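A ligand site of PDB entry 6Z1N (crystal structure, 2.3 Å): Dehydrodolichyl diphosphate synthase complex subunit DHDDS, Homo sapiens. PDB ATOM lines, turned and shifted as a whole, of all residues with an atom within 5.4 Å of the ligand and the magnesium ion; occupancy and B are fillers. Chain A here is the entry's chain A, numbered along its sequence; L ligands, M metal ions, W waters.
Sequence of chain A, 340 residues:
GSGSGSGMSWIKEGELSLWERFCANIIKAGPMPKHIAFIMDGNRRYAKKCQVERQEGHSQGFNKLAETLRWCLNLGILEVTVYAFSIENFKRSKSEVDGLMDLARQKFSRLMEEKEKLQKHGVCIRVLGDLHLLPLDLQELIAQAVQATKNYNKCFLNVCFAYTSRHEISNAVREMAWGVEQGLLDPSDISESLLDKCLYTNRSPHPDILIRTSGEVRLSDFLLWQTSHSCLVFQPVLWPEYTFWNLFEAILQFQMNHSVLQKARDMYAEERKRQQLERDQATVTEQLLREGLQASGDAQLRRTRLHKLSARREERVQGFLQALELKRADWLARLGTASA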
ATOM      1  N   TRP A  10      11.869  36.224  20.833  1.00  0.00           N
ATOM      2  CA  TRP A  10      12.999  35.458  20.327  1.00  0.00           C
ATOM      3  C   TRP A  10      14.032  35.004  21.379  1.00  0.00           C
ATOM      4  O   TRP A  10      15.130  34.618  20.982  1.00  0.00           O
ATOM      5  CB  TRP A  10      13.728  36.254  19.249  1.00  0.00           C
ATOM      6  CG  TRP A  10      13.412  35.836  17.849  1.00  0.00           C
ATOM      7  CD1 TRP A  10      12.301  36.149  17.126  1.00  0.00           C
ATOM      8  CD2 TRP A  10      14.246  35.061  16.979  1.00  0.00           C
ATOM      9  NE1 TRP A  10      12.383  35.611  15.870  1.00  0.00           N
ATOM     10  CE2 TRP A  10      13.563  34.935  15.754  1.00  0.00           C
ATOM     11  CE3 TRP A  10      15.497  34.453  17.115  1.00  0.00           C
ATOM     12  CZ2 TRP A  10      14.096  34.221  14.672  1.00  0.00           C
ATOM     13  CZ3 TRP A  10      16.013  33.748  16.047  1.00  0.00           C
ATOM     14  CH2 TRP A  10      15.319  33.638  14.847  1.00  0.00           C
ATOM     15  N   MET A  40      20.867  21.984  18.112  1.00  0.00           N
ATOM     16  CA  MET A  40      19.549  21.753  18.695  1.00  0.00           C
ATOM     17  C   MET A  40      18.923  20.513  18.060  1.00  0.00           C
ATOM     18  O   MET A  40      18.181  20.600  17.080  1.00  0.00           O
ATOM     19  CB  MET A  40      18.652  22.972  18.501  1.00  0.00           C
ATOM     20  CG  MET A  40      19.270  24.287  18.944  1.00  0.00           C
ATOM     21  SD  MET A  40      18.162  25.681  18.632  1.00  0.00           S
ATOM     22  CE  MET A  40      18.271  25.791  16.840  1.00  0.00           C
ATOM     23  N   ASP A  41      19.190  19.357  18.646  1.00  0.00           N
ATOM     24  CA  ASP A  41      18.838  18.082  18.029  1.00  0.00           C
ATOM     25  C   ASP A  41      17.806  17.335  18.864  1.00  0.00           C
ATOM     26  O   ASP A  41      17.765  17.449  20.098  1.00  0.00           O
ATOM     27  CB  ASP A  41      20.100  17.233  17.852  1.00  0.00           C
ATOM     28  CG  ASP A  41      19.907  16.124  16.853  1.00  0.00           C
ATOM     29  OD1 ASP A  41      18.836  16.081  16.218  1.00  0.00           O
ATOM     30  OD2 ASP A  41      20.834  15.288  16.724  1.00  0.00           O
ATOM     31  N   GLY A  42      16.963  16.550  18.180  1.00  0.00           N
ATOM     32  CA  GLY A  42      15.989  15.685  18.827  1.00  0.00           C
ATOM     33  C   GLY A  42      14.554  16.177  18.809  1.00  0.00           C
ATOM     34  O   GLY A  42      13.723  15.630  19.560  1.00  0.00           O
ATOM     35  N   ASN A  43      14.229  17.180  17.987  1.00  0.00           N
ATOM     36  CA  ASN A  43      12.864  17.713  17.943  1.00  0.00           C
ATOM     37  C   ASN A  43      11.860  16.660  17.509  1.00  0.00           C
ATOM     38  O   ASN A  43      10.776  16.546  18.091  1.00  0.00           O
ATOM     39  CB  ASN A  43      12.819  18.906  16.993  1.00  0.00           C
ATOM     40  CG  ASN A  43      13.568  20.109  17.518  1.00  0.00           C
ATOM     41  OD1 ASN A  43      14.069  20.101  18.633  1.00  0.00           O
ATOM     42  ND2 ASN A  43      13.661  21.151  16.695  1.00  0.00           N
ATOM     43  N   ARG A  44      12.201  15.872  16.478  1.00  0.00           N
ATOM     44  CA  ARG A  44      11.238  14.920  15.940  1.00  0.00           C
ATOM     45  C   ARG A  44      11.007  13.761  16.903  1.00  0.00           C
ATOM     46  O   ARG A  44       9.866  13.346  17.121  1.00  0.00           O
ATOM     47  CB  ARG A  44      11.697  14.424  14.568  1.00  0.00           C
ATOM     48  CG  ARG A  44      11.742  15.517  13.486  1.00  0.00           C
ATOM     49  CD  ARG A  44      12.094  14.947  12.110  1.00  0.00           C
ATOM     50  NE  ARG A  44      13.426  14.336  12.094  1.00  0.00           N
ATOM     51  CZ  ARG A  44      14.060  13.949  10.987  1.00  0.00           C
ATOM     52  NH1 ARG A  44      13.492  14.099   9.805  1.00  0.00           N
ATOM     53  NH2 ARG A  44      15.271  13.397  11.076  1.00  0.00           N
ATOM     54  N   ARG A  45      12.082  13.226  17.488  1.00  0.00           N
ATOM     55  CA  ARG A  45      11.935  12.178  18.492  1.00  0.00           C
ATOM     56  C   ARG A  45      11.076  12.667  19.648  1.00  0.00           C
ATOM     57  O   ARG A  45      10.266  11.907  20.207  1.00  0.00           O
ATOM     58  CB  ARG A  45      13.291  11.726  19.012  1.00  0.00           C
ATOM     59  CG  ARG A  45      13.995  10.652  18.186  1.00  0.00           C
ATOM     60  CD  ARG A  45      15.474  10.582  18.552  1.00  0.00           C
ATOM     61  NE  ARG A  45      16.265  11.625  17.877  1.00  0.00           N
ATOM     62  CZ  ARG A  45      17.552  11.842  18.078  1.00  0.00           C
ATOM     63  NH1 ARG A  45      18.228  11.088  18.942  1.00  0.00           N
ATOM     64  NH2 ARG A  45      18.191  12.807  17.422  1.00  0.00           N
ATOM     65  N   TYR A  46      11.234  13.943  20.029  1.00  0.00           N
ATOM     66  CA  TYR A  46      10.422  14.520  21.097  1.00  0.00           C
ATOM     67  C   TYR A  46       8.958  14.587  20.702  1.00  0.00           C
ATOM     68  O   TYR A  46       8.070  14.329  21.529  1.00  0.00           O
ATOM     69  CB  TYR A  46      10.957  15.909  21.446  1.00  0.00           C
ATOM     70  CG  TYR A  46      10.008  16.747  22.272  1.00  0.00           C
ATOM     71  CD1 TYR A  46       9.965  16.629  23.655  1.00  0.00           C
ATOM     72  CD2 TYR A  46       9.169  17.672  21.663  1.00  0.00           C
ATOM     73  CE1 TYR A  46       9.097  17.415  24.418  1.00  0.00           C
ATOM     74  CE2 TYR A  46       8.297  18.447  22.407  1.00  0.00           C
ATOM     75  CZ  TYR A  46       8.261  18.319  23.784  1.00  0.00           C
ATOM     76  OH  TYR A  46       7.397  19.102  24.506  1.00  0.00           O
ATOM     77  N   HIS A  58       9.160  21.030  16.332  1.00  0.00           N
ATOM     78  CA  HIS A  58      10.049  22.117  15.901  1.00  0.00           C
ATOM     79  C   HIS A  58       9.656  23.433  16.539  1.00  0.00           C
ATOM     80  O   HIS A  58      10.521  24.235  16.905  1.00  0.00           O
ATOM     81  CB  HIS A  58      10.038  22.222  14.381  1.00  0.00           C
ATOM     82  CG  HIS A  58      10.781  21.127  13.687  1.00  0.00           C
ATOM     83  ND1 HIS A  58      11.996  20.648  14.129  1.00  0.00           N
ATOM     84  CD2 HIS A  58      10.474  20.406  12.575  1.00  0.00           C
ATOM     85  CE1 HIS A  58      12.402  19.684  13.322  1.00  0.00           C
ATOM     86  NE2 HIS A  58      11.500  19.525  12.375  1.00  0.00           N
ATOM     87  N   GLY A  61      10.778  23.367  19.916  1.00  0.00           N
ATOM     88  CA  GLY A  61      12.220  23.566  19.859  1.00  0.00           C
ATOM     89  C   GLY A  61      12.602  25.030  19.739  1.00  0.00           C
ATOM     90  O   GLY A  61      13.604  25.474  20.321  1.00  0.00           O
ATOM     91  N   PHE A  62      11.811  25.808  19.001  1.00  0.00           N
ATOM     92  CA  PHE A  62      12.078  27.241  18.959  1.00  0.00           C
ATOM     93  C   PHE A  62      11.847  27.884  20.321  1.00  0.00           C
ATOM     94  O   PHE A  62      12.624  28.753  20.733  1.00  0.00           O
ATOM     95  CB  PHE A  62      11.203  27.940  17.906  1.00  0.00           C
ATOM     96  CG  PHE A  62      11.391  29.423  17.917  1.00  0.00           C
ATOM     97  CD1 PHE A  62      12.442  30.005  17.217  1.00  0.00           C
ATOM     98  CD2 PHE A  62      10.564  30.239  18.670  1.00  0.00           C
ATOM     99  CE1 PHE A  62      12.646  31.380  17.240  1.00  0.00           C
ATOM    100  CE2 PHE A  62      10.755  31.615  18.711  1.00  0.00           C
ATOM    101  CZ  PHE A  62      11.801  32.186  17.992  1.00  0.00           C
ATOM    102  N   LEU A  65      14.841  27.415  22.409  1.00  0.00           N
ATOM    103  CA  LEU A  65      15.909  28.348  22.040  1.00  0.00           C
ATOM    104  C   LEU A  65      15.730  29.688  22.741  1.00  0.00           C
ATOM    105  O   LEU A  65      16.680  30.244  23.312  1.00  0.00           O
ATOM    106  CB  LEU A  65      15.947  28.529  20.521  1.00  0.00           C
ATOM    107  CG  LEU A  65      16.707  29.716  19.915  1.00  0.00           C
ATOM    108  CD1 LEU A  65      18.124  29.834  20.439  1.00  0.00           C
ATOM    109  CD2 LEU A  65      16.718  29.626  18.391  1.00  0.00           C
ATOM    110  N   TYR A  83      22.512  25.890  15.651  1.00  0.00           N
ATOM    111  CA  TYR A  83      22.356  25.227  14.355  1.00  0.00           C
ATOM    112  C   TYR A  83      20.864  25.047  14.109  1.00  0.00           C
ATOM    113  O   TYR A  83      20.250  24.097  14.618  1.00  0.00           O
ATOM    114  CB  TYR A  83      23.084  23.883  14.355  1.00  0.00           C
ATOM    115  CG  TYR A  83      23.540  23.411  12.985  1.00  0.00           C
ATOM    116  CD1 TYR A  83      24.239  22.211  12.842  1.00  0.00           C
ATOM    117  CD2 TYR A  83      23.285  24.151  11.838  1.00  0.00           C
ATOM    118  CE1 TYR A  83      24.670  21.768  11.607  1.00  0.00           C
ATOM    119  CE2 TYR A  83      23.726  23.732  10.589  1.00  0.00           C
ATOM    120  CZ  TYR A  83      24.413  22.530  10.486  1.00  0.00           C
ATOM    121  OH  TYR A  83      24.850  22.075   9.245  1.00  0.00           O
ATOM    122  N   ALA A  84      20.265  25.958  13.346  1.00  0.00           N
ATOM    123  CA  ALA A  84      18.827  25.920  13.136  1.00  0.00           C
ATOM    124  C   ALA A  84      18.421  25.142  11.900  1.00  0.00           C
ATOM    125  O   ALA A  84      17.348  24.517  11.895  1.00  0.00           O
ATOM    126  CB  ALA A  84      18.273  27.353  13.056  1.00  0.00           C
ATOM    127  N   PHE A  85      19.228  25.149  10.838  1.00  0.00           N
ATOM    128  CA  PHE A  85      18.851  24.440   9.611  1.00  0.00           C
ATOM    129  C   PHE A  85      20.094  24.168   8.790  1.00  0.00           C
ATOM    130  O   PHE A  85      20.755  25.114   8.325  1.00  0.00           O
ATOM    131  CB  PHE A  85      17.829  25.264   8.798  1.00  0.00           C
ATOM    132  CG  PHE A  85      17.208  24.488   7.651  1.00  0.00           C
ATOM    133  CD1 PHE A  85      17.783  24.515   6.392  1.00  0.00           C
ATOM    134  CD2 PHE A  85      16.074  23.706   7.856  1.00  0.00           C
ATOM    135  CE1 PHE A  85      17.238  23.796   5.343  1.00  0.00           C
ATOM    136  CE2 PHE A  85      15.505  22.988   6.811  1.00  0.00           C
ATOM    137  CZ  PHE A  85      16.097  23.026   5.554  1.00  0.00           C
ATOM    138  N   ASN A  89      19.560  19.425   5.541  1.00  0.00           N
ATOM    139  CA  ASN A  89      18.148  19.323   5.886  1.00  0.00           C
ATOM    140  C   ASN A  89      17.241  19.614   4.706  1.00  0.00           C
ATOM    141  O   ASN A  89      16.049  19.267   4.744  1.00  0.00           O
ATOM    142  CB  ASN A  89      17.802  20.265   7.032  1.00  0.00           C
ATOM    143  CG  ASN A  89      18.461  19.870   8.323  1.00  0.00           C
ATOM    144  OD1 ASN A  89      18.748  20.715   9.173  1.00  0.00           O
ATOM    145  ND2 ASN A  89      18.742  18.579   8.472  1.00  0.00           N
ATOM    146  N   ARG A  92      15.205  16.703   3.483  1.00  0.00           N
ATOM    147  CA  ARG A  92      14.008  16.217   4.143  1.00  0.00           C
ATOM    148  C   ARG A  92      12.779  16.432   3.251  1.00  0.00           C
ATOM    149  O   ARG A  92      12.842  17.056   2.188  1.00  0.00           O
ATOM    150  CB  ARG A  92      13.838  16.915   5.494  1.00  0.00           C
ATOM    151  CG  ARG A  92      14.773  16.353   6.533  1.00  0.00           C
ATOM    152  CD  ARG A  92      14.692  17.104   7.835  1.00  0.00           C
ATOM    153  NE  ARG A  92      15.778  16.714   8.733  1.00  0.00           N
ATOM    154  CZ  ARG A  92      15.743  16.889  10.048  1.00  0.00           C
ATOM    155  NH1 ARG A  92      14.671  17.430  10.609  1.00  0.00           N
ATOM    156  NH2 ARG A  92      16.777  16.506  10.794  1.00  0.00           N
ATOM    157  N   GLU A  96       8.027  18.653   5.557  1.00  0.00           N
ATOM    158  CA  GLU A  96       8.777  19.066   6.738  1.00  0.00           C
ATOM    159  C   GLU A  96       9.593  20.320   6.457  1.00  0.00           C
ATOM    160  O   GLU A  96       9.683  21.204   7.314  1.00  0.00           O
ATOM    161  CB  GLU A  96       9.673  17.935   7.237  1.00  0.00           C
ATOM    162  CG  GLU A  96      10.418  18.325   8.520  1.00  0.00           C
ATOM    163  CD  GLU A  96      11.289  17.228   9.110  1.00  0.00           C
ATOM    164  OE1 GLU A  96      11.292  16.090   8.578  1.00  0.00           O
ATOM    165  OE2 GLU A  96      11.976  17.531  10.106  1.00  0.00           O
ATOM    166  N   LEU A 100       9.366  23.936   8.339  1.00  0.00           N
ATOM    167  CA  LEU A 100      10.475  24.673   8.927  1.00  0.00           C
ATOM    168  C   LEU A 100      10.612  26.072   8.323  1.00  0.00           C
ATOM    169  O   LEU A 100      10.875  27.032   9.039  1.00  0.00           O
ATOM    170  CB  LEU A 100      11.775  23.875   8.766  1.00  0.00           C
ATOM    171  CG  LEU A 100      11.897  22.671   9.704  1.00  0.00           C
ATOM    172  CD1 LEU A 100      12.810  21.609   9.124  1.00  0.00           C
ATOM    173  CD2 LEU A 100      12.383  23.097  11.099  1.00  0.00           C
ATOM    174  N   LEU A 103       7.894  28.231   9.865  1.00  0.00           N
ATOM    175  CA  LEU A 103       8.299  28.619  11.220  1.00  0.00           C
ATOM    176  C   LEU A 103       9.273  29.797  11.165  1.00  0.00           C
ATOM    177  O   LEU A 103       9.087  30.793  11.865  1.00  0.00           O
ATOM    178  CB  LEU A 103       8.918  27.422  11.939  1.00  0.00           C
ATOM    179  CG  LEU A 103       9.184  27.597  13.439  1.00  0.00           C
ATOM    180  CD1 LEU A 103       7.870  27.837  14.190  1.00  0.00           C
ATOM    181  CD2 LEU A 103       9.906  26.380  13.997  1.00  0.00           C
ATOM    182  N   ALA A 104      10.297  29.687  10.323  1.00  0.00           N
ATOM    183  CA  ALA A 104      11.283  30.750  10.208  1.00  0.00           C
ATOM    184  C   ALA A 104      10.654  32.041   9.704  1.00  0.00           C
ATOM    185  O   ALA A 104      11.009  33.130  10.161  1.00  0.00           O
ATOM    186  CB  ALA A 104      12.420  30.315   9.281  1.00  0.00           C
ATOM    187  N   LYS A 107       8.822  33.313  12.928  1.00  0.00           N
ATOM    188  CA  LYS A 107       9.639  33.797  14.042  1.00  0.00           C
ATOM    189  C   LYS A 107      10.420  35.045  13.648  1.00  0.00           C
ATOM    190  O   LYS A 107      10.373  36.059  14.353  1.00  0.00           O
ATOM    191  CB  LYS A 107      10.557  32.689  14.539  1.00  0.00           C
ATOM    192  CG  LYS A 107       9.783  31.542  15.173  1.00  0.00           C
ATOM    193  CD  LYS A 107       8.655  32.065  16.067  1.00  0.00           C
ATOM    194  CE  LYS A 107       7.629  30.987  16.379  1.00  0.00           C
ATOM    195  NZ  LYS A 107       6.626  31.421  17.390  1.00  0.00           N
ATOM    196  N   PHE A 108      11.124  34.997  12.503  1.00  0.00           N
ATOM    197  CA  PHE A 108      11.419  36.253  11.837  1.00  0.00           C
ATOM    198  C   PHE A 108      10.067  36.911  11.547  1.00  0.00           C
ATOM    199  O   PHE A 108       9.029  36.315  11.807  1.00  0.00           O
ATOM    200  CB  PHE A 108      12.246  36.028  10.567  1.00  0.00           C
ATOM    201  CG  PHE A 108      13.596  35.382  10.800  1.00  0.00           C
ATOM    202  CD1 PHE A 108      14.664  36.122  11.272  1.00  0.00           C
ATOM    203  CD2 PHE A 108      13.788  34.028  10.553  1.00  0.00           C
ATOM    204  CE1 PHE A 108      15.901  35.530  11.495  1.00  0.00           C
ATOM    205  CE2 PHE A 108      15.019  33.428  10.766  1.00  0.00           C
ATOM    206  CZ  PHE A 108      16.082  34.176  11.235  1.00  0.00           C
ATOM    207  N   VAL A 159      22.195  32.698  14.239  1.00  0.00           N
ATOM    208  CA  VAL A 159      21.296  31.626  13.793  1.00  0.00           C
ATOM    209  C   VAL A 159      21.880  31.044  12.515  1.00  0.00           C
ATOM    210  O   VAL A 159      21.854  31.681  11.459  1.00  0.00           O
ATOM    211  CB  VAL A 159      19.865  32.134  13.570  1.00  0.00           C
ATOM    212  CG1 VAL A 159      18.996  30.993  13.095  1.00  0.00           C
ATOM    213  CG2 VAL A 159      19.319  32.749  14.847  1.00  0.00           C
ATOM    214  N   PHE A 161      21.554  29.016   9.500  1.00  0.00           N
ATOM    215  CA  PHE A 161      20.387  28.617   8.719  1.00  0.00           C
ATOM    216  C   PHE A 161      20.844  28.368   7.298  1.00  0.00           C
ATOM    217  O   PHE A 161      21.549  29.209   6.724  1.00  0.00           O
ATOM    218  CB  PHE A 161      19.311  29.719   8.751  1.00  0.00           C
ATOM    219  CG  PHE A 161      17.896  29.183   8.749  1.00  0.00           C
ATOM    220  CD1 PHE A 161      17.297  28.770   7.569  1.00  0.00           C
ATOM    221  CD2 PHE A 161      17.166  29.132   9.926  1.00  0.00           C
ATOM    222  CE1 PHE A 161      16.005  28.302   7.566  1.00  0.00           C
ATOM    223  CE2 PHE A 161      15.865  28.659   9.921  1.00  0.00           C
ATOM    224  CZ  PHE A 161      15.292  28.240   8.750  1.00  0.00           C
ATOM    225  N   ARG A 212      25.691  19.510  21.899  1.00  0.00           N
ATOM    226  CA  ARG A 212      24.763  18.813  21.011  1.00  0.00           C
ATOM    227  C   ARG A 212      23.837  17.925  21.835  1.00  0.00           C
ATOM    228  O   ARG A 212      24.310  17.073  22.585  1.00  0.00           O
ATOM    229  CB  ARG A 212      25.489  17.963  19.958  1.00  0.00           C
ATOM    230  CG  ARG A 212      24.533  17.044  19.189  1.00  0.00           C
ATOM    231  CD  ARG A 212      25.063  16.706  17.810  1.00  0.00           C
ATOM    232  NE  ARG A 212      24.003  16.236  16.914  1.00  0.00           N
ATOM    233  CZ  ARG A 212      24.195  15.908  15.635  1.00  0.00           C
ATOM    234  NH1 ARG A 212      25.412  15.987  15.114  1.00  0.00           N
ATOM    235  NH2 ARG A 212      23.179  15.507  14.878  1.00  0.00           N
ATOM    236  N   SER A 214      20.334  15.234  22.301  1.00  0.00           N
ATOM    237  CA  SER A 214      20.010  13.865  21.919  1.00  0.00           C
ATOM    238  C   SER A 214      21.267  13.012  22.040  1.00  0.00           C
ATOM    239  O   SER A 214      22.325  13.499  22.442  1.00  0.00           O
ATOM    240  CB  SER A 214      19.368  13.788  20.519  1.00  0.00           C
ATOM    241  OG  SER A 214      20.267  14.149  19.485  1.00  0.00           O
ATOM    242  N   TRP A 239      16.324  18.054  22.578  1.00  0.00           N
ATOM    243  CA  TRP A 239      16.434  19.529  22.616  1.00  0.00           C
ATOM    244  C   TRP A 239      15.202  20.204  23.189  1.00  0.00           C
ATOM    245  O   TRP A 239      15.386  21.082  24.080  1.00  0.00           O
ATOM    246  CB  TRP A 239      16.731  20.087  21.220  1.00  0.00           C
ATOM    247  CG  TRP A 239      16.591  21.598  21.212  1.00  0.00           C
ATOM    248  CD1 TRP A 239      15.602  22.322  20.615  1.00  0.00           C
ATOM    249  CD2 TRP A 239      17.444  22.546  21.864  1.00  0.00           C
ATOM    250  NE1 TRP A 239      15.789  23.663  20.846  1.00  0.00           N
ATOM    251  CE2 TRP A 239      16.916  23.836  21.607  1.00  0.00           C
ATOM    252  CE3 TRP A 239      18.601  22.448  22.633  1.00  0.00           C
ATOM    253  CZ2 TRP A 239      17.507  24.994  22.087  1.00  0.00           C
ATOM    254  CZ3 TRP A 239      19.191  23.608  23.123  1.00  0.00           C
ATOM    255  CH2 TRP A 239      18.637  24.864  22.848  1.00  0.00           C
HETATM  256  C1  LIG L   1      16.970  19.050  14.634  1.00  0.00           C
HETATM  257  O1  LIG L   1      16.345  18.017  15.344  1.00  0.00           O
HETATM  258  C2  LIG L   1      16.122  20.320  14.649  1.00  0.00           C
HETATM  259  C3  LIG L   1      15.942  21.025  13.550  1.00  0.00           C
HETATM  260  C4  LIG L   1      16.570  20.552  12.241  1.00  0.00           C
HETATM  261  C5  LIG L   1      15.109  22.309  13.576  1.00  0.00           C
HETATM  262  C6  LIG L   1      15.793  23.365  14.457  1.00  0.00           C
HETATM  263  C7  LIG L   1      15.015  24.685  14.378  1.00  0.00           C
HETATM  264  C8  LIG L   1      14.577  25.315  15.453  1.00  0.00           C
HETATM  265  C9  LIG L   1      14.838  24.737  16.843  1.00  0.00           C
HETATM  266  C10 LIG L   1      13.794  26.628  15.333  1.00  0.00           C
HETATM  267  C11 LIG L   1      13.647  27.098  13.882  1.00  0.00           C
HETATM  268  C12 LIG L   1      14.658  28.210  13.673  1.00  0.00           C
HETATM  269  C13 LIG L   1      14.293  29.465  13.526  1.00  0.00           C
HETATM  270  C14 LIG L   1      15.361  30.538  13.321  1.00  0.00           C
HETATM  271  C15 LIG L   1      12.819  29.862  13.537  1.00  0.00           C
HETATM  272  P1  LIG L   1      15.671  16.830  14.427  1.00  0.00           P
HETATM  273  O2  LIG L   1      14.603  17.425  13.529  1.00  0.00           O
HETATM  274  O3  LIG L   1      16.724  16.194  13.569  1.00  0.00           O
HETATM  275  O4  LIG L   1      14.989  15.723  15.421  1.00  0.00           O
HETATM  276  P2  LIG L   1      15.454  14.150  15.457  1.00  0.00           P
HETATM  277  O5  LIG L   1      14.938  13.443  14.219  1.00  0.00           O
HETATM  278  O6  LIG L   1      16.956  14.060  15.473  1.00  0.00           O
HETATM  279  O7  LIG L   1      14.863  13.537  16.705  1.00  0.00           O
HETATM  280 MG    MG M   1      18.397  15.078  14.474  1.00  0.00          MG
HETATM  281  O   HOH W   1      19.976  16.045  13.426  1.00  0.00           O
HETATM  282  O   HOH W   2      18.215  13.815  12.724  1.00  0.00           O
HETATM  283  O   HOH W   3      19.915  13.865  15.084  1.00  0.00           O
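The backbone NH of Arg 45 is in hydrogen-bond range of an oxygen (O7) of the ligand.
The guanidinium group (NE) of Arg 45 lies within salt-bridge range of an oxygen (O7) of the ligand, 2.6 Å away.
N of Arg 44 lies within hydrogen-bond range of O4 of the ligand, at 3.0 Å.
An oxygen (O5) of the ligand is in salt-bridge range of the guanidinium group (NE) of Arg 44, 2.8 Å away.
The guanidinium group (NH1) of Arg 92 is in salt-bridge range of an oxygen (O2) of the ligand, at 2.9 Å.
The backbone NH of Asn 43 lies within hydrogen-bond range of an oxygen (O4) of the ligand.
The backbone NH of Gly 42 lies within hydrogen-bond range of an oxygen (O1) of the ligand (3.3 Å).
OD2 of Asp 41 lies within salt-bridge range of NH2 of Arg 212 (3.0 Å).
The side-chain carboxylate of Asp 41 sits at hydrogen-bond distance from the side-chain hydroxyl of Ser 214, 3.0 Å away.
The guanidinium group (NH2) of Arg 45 lies within hydrogen-bond range of the side-chain hydroxyl (OG) of Ser 214 (3.2 Å).
NH1 of Arg 92 lies within salt-bridge range of OE2 of Glu 96, 2.7 Å away.
A ring nitrogen (ND1) of His 58 is in hydrogen-bond range of the side-chain amide nitrogen of Asn 43 (3.1 Å).
A ring nitrogen (NE2) of His 58 is in hydrogen-bond range of the side-chain carboxylate (OE2) of Glu 96 (3.1 Å).
The backbone carbonyl oxygen of Lys 107 is in hydrogen-bond range of the indole nitrogen of Trp 10 (2.6 Å).
NE1 of Trp 239 is in hydrogen-bond range of O of Gly 61 (2.9 Å).
Trp 10 touches the ligand (CH2 to C14, 3.5 Å).
O of Met 40 touches C1 of the ligand, 3.1 Å away.
His 58 touches the ligand.
C of Gly 61 touches C9 of the ligand, 3.7 Å away.
Phe 62 touches the ligand (CD1 to C15, 3.7 Å).
Ala 84 touches the ligand.
OD1 of Asn 89 touches C4 of the ligand (3.8 Å).
CD2 of Leu 100 touches C5 of the ligand, 3.8 Å away.
CD2 of Leu 103 touches C11 of the ligand (3.8 Å).
Ala 104 touches the ligand (CA to C15, 3.8 Å).
Lys 107 touches the ligand.
Phe 108 touches the ligand.
Val 159 touches the ligand.
Phe 161 touches the ligand (CE2 to C14, 3.9 Å).
Hydrophobic or aromatic side chains that line the ligand: Trp 10, Met 40, His 58, Phe 62, Ala 84, Leu 100, Leu 103, Phe 108, Val 159 and Phe 161.
Along chain A the residues within 4 Å of the ligand span positions 10 to 161.
The nearest printed residue that does not touch the ligand is Trp 239 (4.3 Å).
Residues that only touch the magnesium ion: Arg 45 (3.7 Å).
Of the 28 residues printed, 2 come within 4 Å of the magnesium ion.
The magnesium ion is bound by an oxygen (O6) of the ligand (2.0 Å), water W3 (2.0 Å), the side-chain carboxylate of Asp 41 (2.1 Å), water W1 (2.1 Å), water W2 (2.2 Å) and an oxygen (O3) of the ligand (2.2 Å).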
